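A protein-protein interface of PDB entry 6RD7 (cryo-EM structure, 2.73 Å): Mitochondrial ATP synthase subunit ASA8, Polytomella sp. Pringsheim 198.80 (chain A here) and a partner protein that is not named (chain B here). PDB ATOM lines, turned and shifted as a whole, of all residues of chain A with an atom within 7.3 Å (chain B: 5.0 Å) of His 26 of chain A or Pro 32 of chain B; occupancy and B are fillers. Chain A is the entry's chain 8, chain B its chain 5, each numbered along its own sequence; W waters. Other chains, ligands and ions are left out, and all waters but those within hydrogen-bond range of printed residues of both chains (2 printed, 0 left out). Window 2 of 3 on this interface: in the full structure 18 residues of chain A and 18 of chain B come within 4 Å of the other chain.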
ATOM      1  N   ASN A  23      29.389  14.821 -20.110  1.00  0.00           N
ATOM      2  CA  ASN A  23      29.164  15.777 -21.182  1.00  0.00           C
ATOM      3  C   ASN A  23      29.063  17.185 -20.619  1.00  0.00           C
ATOM      4  O   ASN A  23      28.456  17.408 -19.569  1.00  0.00           O
ATOM      5  CB  ASN A  23      27.901  15.418 -21.958  1.00  0.00           C
ATOM      6  CG  ASN A  23      27.854  16.073 -23.316  1.00  0.00           C
ATOM      7  OD1 ASN A  23      28.793  16.752 -23.720  1.00  0.00           O
ATOM      8  ND2 ASN A  23      26.762  15.870 -24.033  1.00  0.00           N
ATOM      9  N   VAL A  24      29.680  18.133 -21.314  1.00  0.00           N
ATOM     10  CA  VAL A  24      29.640  19.537 -20.923  1.00  0.00           C
ATOM     11  C   VAL A  24      28.252  20.071 -21.249  1.00  0.00           C
ATOM     12  O   VAL A  24      27.813  19.984 -22.403  1.00  0.00           O
ATOM     13  CB  VAL A  24      30.737  20.346 -21.631  1.00  0.00           C
ATOM     14  CG1 VAL A  24      30.477  21.831 -21.497  1.00  0.00           C
ATOM     15  CG2 VAL A  24      32.093  19.993 -21.060  1.00  0.00           C
ATOM     16  N   PRO A  25      27.526  20.611 -20.278  1.00  0.00           N
ATOM     17  CA  PRO A  25      26.185  21.119 -20.562  1.00  0.00           C
ATOM     18  C   PRO A  25      26.215  22.470 -21.252  1.00  0.00           C
ATOM     19  O   PRO A  25      27.108  23.292 -21.042  1.00  0.00           O
ATOM     20  CB  PRO A  25      25.557  21.234 -19.170  1.00  0.00           C
ATOM     21  CG  PRO A  25      26.695  21.447 -18.272  1.00  0.00           C
ATOM     22  CD  PRO A  25      27.859  20.706 -18.849  1.00  0.00           C
ATOM     23  N   HIS A  26      25.228  22.678 -22.092  1.00  0.00           N
ATOM     24  CA  HIS A  26      24.961  24.005 -22.605  1.00  0.00           C
ATOM     25  C   HIS A  26      24.369  24.859 -21.485  1.00  0.00           C
ATOM     26  O   HIS A  26      23.745  24.325 -20.566  1.00  0.00           O
ATOM     27  CB  HIS A  26      23.996  23.927 -23.782  1.00  0.00           C
ATOM     28  CG  HIS A  26      23.844  25.212 -24.528  1.00  0.00           C
ATOM     29  ND1 HIS A  26      24.731  25.619 -25.495  1.00  0.00           N
ATOM     30  CD2 HIS A  26      22.918  26.192 -24.435  1.00  0.00           C
ATOM     31  CE1 HIS A  26      24.356  26.792 -25.968  1.00  0.00           C
ATOM     32  NE2 HIS A  26      23.258  27.162 -25.340  1.00  0.00           N
ATOM     33  N   PRO A  27      24.592  26.187 -21.510  1.00  0.00           N
ATOM     34  CA  PRO A  27      23.966  27.074 -20.514  1.00  0.00           C
ATOM     35  C   PRO A  27      22.443  27.036 -20.451  1.00  0.00           C
ATOM     36  O   PRO A  27      21.863  27.368 -19.416  1.00  0.00           O
ATOM     37  CB  PRO A  27      24.450  28.459 -20.950  1.00  0.00           C
ATOM     38  CG  PRO A  27      25.761  28.209 -21.563  1.00  0.00           C
ATOM     39  CD  PRO A  27      25.743  26.837 -22.162  1.00  0.00           C
ATOM     40  N   PHE A  28      21.786  26.640 -21.541  1.00  0.00           N
ATOM     41  CA  PHE A  28      20.335  26.512 -21.524  1.00  0.00           C
ATOM     42  C   PHE A  28      19.912  25.227 -20.830  1.00  0.00           C
ATOM     43  O   PHE A  28      18.848  25.169 -20.207  1.00  0.00           O
ATOM     44  CB  PHE A  28      19.777  26.545 -22.945  1.00  0.00           C
ATOM     45  CG  PHE A  28      19.889  27.881 -23.628  1.00  0.00           C
ATOM     46  CD1 PHE A  28      20.155  29.034 -22.915  1.00  0.00           C
ATOM     47  CD2 PHE A  28      19.718  27.973 -24.993  1.00  0.00           C
ATOM     48  CE1 PHE A  28      20.251  30.245 -23.549  1.00  0.00           C
ATOM     49  CE2 PHE A  28      19.817  29.182 -25.629  1.00  0.00           C
ATOM     50  CZ  PHE A  28      20.079  30.318 -24.904  1.00  0.00           C
ATOM     51  N   GLN A  29      20.729  24.178 -20.941  1.00  0.00           N
ATOM     52  CA  GLN A  29      20.457  22.943 -20.216  1.00  0.00           C
ATOM     53  C   GLN A  29      20.730  23.113 -18.732  1.00  0.00           C
ATOM     54  O   GLN A  29      20.096  22.460 -17.897  1.00  0.00           O
ATOM     55  CB  GLN A  29      21.309  21.809 -20.775  1.00  0.00           C
ATOM     56  CG  GLN A  29      21.183  21.607 -22.256  1.00  0.00           C
ATOM     57  CD  GLN A  29      21.878  20.358 -22.725  1.00  0.00           C
ATOM     58  OE1 GLN A  29      21.277  19.292 -22.797  1.00  0.00           O
ATOM     59  NE2 GLN A  29      23.156  20.482 -23.051  1.00  0.00           N
ATOM     60  N   THR A  30      21.684  23.978 -18.392  1.00  0.00           N
ATOM     61  CA  THR A  30      22.009  24.245 -16.995  1.00  0.00           C
ATOM     62  C   THR A  30      20.875  24.986 -16.300  1.00  0.00           C
ATOM     63  O   THR A  30      20.486  24.636 -15.180  1.00  0.00           O
ATOM     64  CB  THR A  30      23.305  25.056 -16.926  1.00  0.00           C
ATOM     65  OG1 THR A  30      24.390  24.277 -17.438  1.00  0.00           O
ATOM     66  CG2 THR A  30      23.624  25.481 -15.501  1.00  0.00           C
ATOM     67  N   SER A  31      20.305  25.985 -16.965  1.00  0.00           N
ATOM     68  CA  SER A  31      19.408  26.926 -16.316  1.00  0.00           C
ATOM     69  C   SER A  31      18.213  27.206 -17.208  1.00  0.00           C
ATOM     70  O   SER A  31      18.374  27.484 -18.398  1.00  0.00           O
ATOM     71  CB  SER A  31      20.137  28.234 -16.004  1.00  0.00           C
ATOM     72  OG  SER A  31      19.387  29.040 -15.118  1.00  0.00           O
ATOM     73  N   THR A  34      18.364  31.231 -17.573  1.00  0.00           N
ATOM     74  CA  THR A  34      19.245  31.711 -18.631  1.00  0.00           C
ATOM     75  C   THR A  34      18.573  31.598 -19.992  1.00  0.00           C
ATOM     76  O   THR A  34      18.646  32.524 -20.808  1.00  0.00           O
ATOM     77  CB  THR A  34      20.554  30.922 -18.599  1.00  0.00           C
ATOM     78  OG1 THR A  34      21.229  31.182 -17.366  1.00  0.00           O
ATOM     79  CG2 THR A  34      21.465  31.305 -19.745  1.00  0.00           C
ATOM     80  N   LYS A  39      17.009  33.747 -24.454  1.00  0.00           N
ATOM     81  CA  LYS A  39      16.455  33.324 -25.735  1.00  0.00           C
ATOM     82  C   LYS A  39      14.940  33.257 -25.764  1.00  0.00           C
ATOM     83  O   LYS A  39      14.344  33.612 -26.783  1.00  0.00           O
ATOM     84  CB  LYS A  39      17.031  31.964 -26.154  1.00  0.00           C
ATOM     85  CG  LYS A  39      16.795  31.656 -27.624  1.00  0.00           C
ATOM     86  CD  LYS A  39      17.488  30.405 -28.075  1.00  0.00           C
ATOM     87  CE  LYS A  39      18.425  30.698 -29.219  1.00  0.00           C
ATOM     88  NZ  LYS A  39      19.212  29.500 -29.596  1.00  0.00           N
ATOM     89  N   LEU B  26      13.377  21.786 -28.198  1.00  0.00           N
ATOM     90  CA  LEU B  26      14.166  22.032 -29.392  1.00  0.00           C
ATOM     91  C   LEU B  26      15.284  23.020 -29.107  1.00  0.00           C
ATOM     92  O   LEU B  26      16.451  22.723 -29.365  1.00  0.00           O
ATOM     93  CB  LEU B  26      13.265  22.540 -30.510  1.00  0.00           C
ATOM     94  CG  LEU B  26      13.949  22.780 -31.847  1.00  0.00           C
ATOM     95  CD1 LEU B  26      14.542  21.491 -32.374  1.00  0.00           C
ATOM     96  CD2 LEU B  26      12.953  23.351 -32.821  1.00  0.00           C
ATOM     97  N   ASP B  27      14.953  24.177 -28.528  1.00  0.00           N
ATOM     98  CA  ASP B  27      15.921  25.244 -28.302  1.00  0.00           C
ATOM     99  C   ASP B  27      16.983  24.873 -27.278  1.00  0.00           C
ATOM    100  O   ASP B  27      18.107  25.376 -27.341  1.00  0.00           O
ATOM    101  CB  ASP B  27      15.203  26.499 -27.825  1.00  0.00           C
ATOM    102  CG  ASP B  27      14.894  27.451 -28.937  1.00  0.00           C
ATOM    103  OD1 ASP B  27      15.654  27.493 -29.921  1.00  0.00           O
ATOM    104  OD2 ASP B  27      13.892  28.175 -28.817  1.00  0.00           O
ATOM    105  N   THR B  28      16.643  24.015 -26.328  1.00  0.00           N
ATOM    106  CA  THR B  28      17.478  23.775 -25.164  1.00  0.00           C
ATOM    107  C   THR B  28      18.201  22.440 -25.215  1.00  0.00           C
ATOM    108  O   THR B  28      19.391  22.379 -24.903  1.00  0.00           O
ATOM    109  CB  THR B  28      16.607  23.871 -23.904  1.00  0.00           C
ATOM    110  OG1 THR B  28      16.168  25.221 -23.742  1.00  0.00           O
ATOM    111  CG2 THR B  28      17.357  23.483 -22.671  1.00  0.00           C
ATOM    112  N   GLN B  29      17.535  21.377 -25.651  1.00  0.00           N
ATOM    113  CA  GLN B  29      18.127  20.050 -25.652  1.00  0.00           C
ATOM    114  C   GLN B  29      18.555  19.600 -27.042  1.00  0.00           C
ATOM    115  O   GLN B  29      19.611  18.985 -27.192  1.00  0.00           O
ATOM    116  CB  GLN B  29      17.143  19.047 -25.046  1.00  0.00           C
ATOM    117  CG  GLN B  29      16.493  19.529 -23.770  1.00  0.00           C
ATOM    118  CD  GLN B  29      17.442  19.531 -22.598  1.00  0.00           C
ATOM    119  OE1 GLN B  29      17.319  20.345 -21.689  1.00  0.00           O
ATOM    120  NE2 GLN B  29      18.389  18.606 -22.604  1.00  0.00           N
ATOM    121  N   LEU B  30      17.764  19.895 -28.071  1.00  0.00           N
ATOM    122  CA  LEU B  30      18.060  19.344 -29.386  1.00  0.00           C
ATOM    123  C   LEU B  30      18.986  20.253 -30.181  1.00  0.00           C
ATOM    124  O   LEU B  30      19.971  19.778 -30.757  1.00  0.00           O
ATOM    125  CB  LEU B  30      16.762  19.086 -30.144  1.00  0.00           C
ATOM    126  CG  LEU B  30      15.840  18.114 -29.408  1.00  0.00           C
ATOM    127  CD1 LEU B  30      14.419  18.211 -29.914  1.00  0.00           C
ATOM    128  CD2 LEU B  30      16.357  16.696 -29.520  1.00  0.00           C
ATOM    129  N   LEU B  31      18.695  21.559 -30.221  1.00  0.00           N
ATOM    130  CA  LEU B  31      19.507  22.468 -31.032  1.00  0.00           C
ATOM    131  C   LEU B  31      20.940  22.656 -30.540  1.00  0.00           C
ATOM    132  O   LEU B  31      21.823  22.797 -31.397  1.00  0.00           O
ATOM    133  CB  LEU B  31      18.808  23.821 -31.189  1.00  0.00           C
ATOM    134  CG  LEU B  31      17.932  24.008 -32.423  1.00  0.00           C
ATOM    135  CD1 LEU B  31      17.395  25.422 -32.472  1.00  0.00           C
ATOM    136  CD2 LEU B  31      18.713  23.696 -33.674  1.00  0.00           C
ATOM    137  N   PRO B  32      21.259  22.705 -29.204  1.00  0.00           N
ATOM    138  CA  PRO B  32      22.681  22.727 -28.828  1.00  0.00           C
ATOM    139  C   PRO B  32      23.476  21.506 -29.263  1.00  0.00           C
ATOM    140  O   PRO B  32      24.606  21.647 -29.735  1.00  0.00           O
ATOM    141  CB  PRO B  32      22.625  22.838 -27.304  1.00  0.00           C
ATOM    142  CG  PRO B  32      21.462  23.645 -27.082  1.00  0.00           C
ATOM    143  CD  PRO B  32      20.449  23.117 -28.039  1.00  0.00           C
ATOM    144  N   THR B  33      22.880  20.320 -29.148  1.00  0.00           N
ATOM    145  CA  THR B  33      23.532  19.092 -29.597  1.00  0.00           C
ATOM    146  C   THR B  33      23.725  19.089 -31.110  1.00  0.00           C
ATOM    147  O   THR B  33      24.821  18.785 -31.613  1.00  0.00           O
ATOM    148  CB  THR B  33      22.694  17.895 -29.153  1.00  0.00           C
ATOM    149  OG1 THR B  33      22.820  17.719 -27.739  1.00  0.00           O
ATOM    150  CG2 THR B  33      23.122  16.634 -29.852  1.00  0.00           C
ATOM    151  N   ILE B  34      22.665  19.445 -31.843  1.00  0.00           N
ATOM    152  CA  ILE B  34      22.702  19.510 -33.300  1.00  0.00           C
ATOM    153  C   ILE B  34      23.724  20.537 -33.767  1.00  0.00           C
ATOM    154  O   ILE B  34      24.476  20.289 -34.710  1.00  0.00           O
ATOM    155  CB  ILE B  34      21.294  19.815 -33.844  1.00  0.00           C
ATOM    156  CG1 ILE B  34      20.419  18.577 -33.770  1.00  0.00           C
ATOM    157  CG2 ILE B  34      21.329  20.239 -35.281  1.00  0.00           C
ATOM    158  CD1 ILE B  34      18.975  18.891 -33.866  1.00  0.00           C
ATOM    159  N   MET B  35      23.818  21.674 -33.076  1.00  0.00           N
ATOM    160  CA  MET B  35      24.745  22.713 -33.506  1.00  0.00           C
ATOM    161  C   MET B  35      26.180  22.376 -33.150  1.00  0.00           C
ATOM    162  O   MET B  35      27.090  22.756 -33.884  1.00  0.00           O
ATOM    163  CB  MET B  35      24.369  24.068 -32.917  1.00  0.00           C
ATOM    164  CG  MET B  35      23.193  24.736 -33.571  1.00  0.00           C
ATOM    165  SD  MET B  35      23.408  24.831 -35.349  1.00  0.00           S
ATOM    166  CE  MET B  35      22.076  23.790 -35.921  1.00  0.00           C
ATOM    167  N   ARG B  36      26.409  21.661 -32.042  1.00  0.00           N
ATOM    168  CA  ARG B  36      27.755  21.174 -31.750  1.00  0.00           C
ATOM    169  C   ARG B  36      28.230  20.215 -32.828  1.00  0.00           C
ATOM    170  O   ARG B  36      29.300  20.412 -33.427  1.00  0.00           O
ATOM    171  CB  ARG B  36      27.784  20.487 -30.389  1.00  0.00           C
ATOM    172  CG  ARG B  36      27.854  21.425 -29.216  1.00  0.00           C
ATOM    173  CD  ARG B  36      27.595  20.685 -27.931  1.00  0.00           C
ATOM    174  NE  ARG B  36      27.527  21.594 -26.796  1.00  0.00           N
ATOM    175  CZ  ARG B  36      27.743  21.233 -25.539  1.00  0.00           C
ATOM    176  NH1 ARG B  36      27.660  22.130 -24.572  1.00  0.00           N
ATOM    177  NH2 ARG B  36      28.047  19.978 -25.250  1.00  0.00           N
HETATM  178  O   HOH W   1      25.699  17.822 -26.623  1.00  0.00           O
HETATM  179  O   HOH W   2      18.829  27.103 -29.482  1.00  0.00           O
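OD1 of Asn 23 of chain A touches NH2 of Arg 36 of chain B, 3.6 Å away.
Pro 25 of chain A touches Arg 36 of chain B (C to NH1, 3.6 Å).
His 26 of chain A touches Pro 32 of chain B (CG to CG, 3.8 Å).
Arg 36 of chain B touches His 26 of chain A.
O of Asp 27 of chain B touches CD2 of Phe 28 of chain A, at 3.9 Å.
CG2 of Thr 28 of chain B touches O of Phe 28 of chain A (3.3 Å).
CG of Gln 29 of chain A touches O of Thr 28 of chain B, at 3.3 Å.
Lys 39 of chain A touches Asp 27 of chain B (CD to OD1, 3.9 Å).
Pro 32 of chain B touches one residue of chain A.
Of the printed residues of chain A, Thr 28 of chain B touches Phe 28 and Gln 29.
Printed residues of chain B within 4 Å of Pro 25 of chain A: Arg 36 (3.6 Å).
Ser 31 of chain A touches none of the printed residues of chain B.
Thr 34 of chain A touches none of the printed residues of chain B.
The nearest printed residue of chain B that does not touch His 26 of chain A is Thr 28 of chain B (5.0 Å).
The nearest printed residue of chain B that does not touch Gln 29 of chain A is Pro 32 of chain B (4.9 Å).
Water W2 bridges NZ of Lys 39 of chain A (2.4 Å) and O of Asp 27 of chain B (2.8 Å).
Water W1 lies within hydrogen-bond range of OG1 of Thr 33 of chain B (3.1 Å), ND2 of Asn 23 of chain A (3.4 Å) and NH2 of Arg 36 of chain B (3.5 Å).
The backbone carbonyl oxygen (O) of Gln 29 of chain B is in hydrogen-bond range of the side-chain hydroxyl (OG1) of Thr 33 of chain B, at 3.5 Å.
NE2 of Gln 29 of chain A lies close to N of His 26 of chain A (3.2 Å).
The backbone carbonyl oxygen (O) of His 26 of chain A lies within hydrogen-bond range of the side-chain hydroxyl (OG1) of Thr 30 of chain A (3.2 Å).
NE2 of Gln 29 of chain B is in hydrogen-bond range of OE1 of Gln 29 of chain A, 3.0 Å away.
The backbone carbonyl oxygen (O) of Val 24 of chain A sits at hydrogen-bond distance from the guanidinium group (NH2) of Arg 36 of chain B (2.9 Å).
Of the 11 printed residues of chain B, 5 touch a printed residue of chain A.
Among the printed residues, no Asp or Glu carboxylate lies within 4 Å of a Lys or Arg side-chain nitrogen of the other chain.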
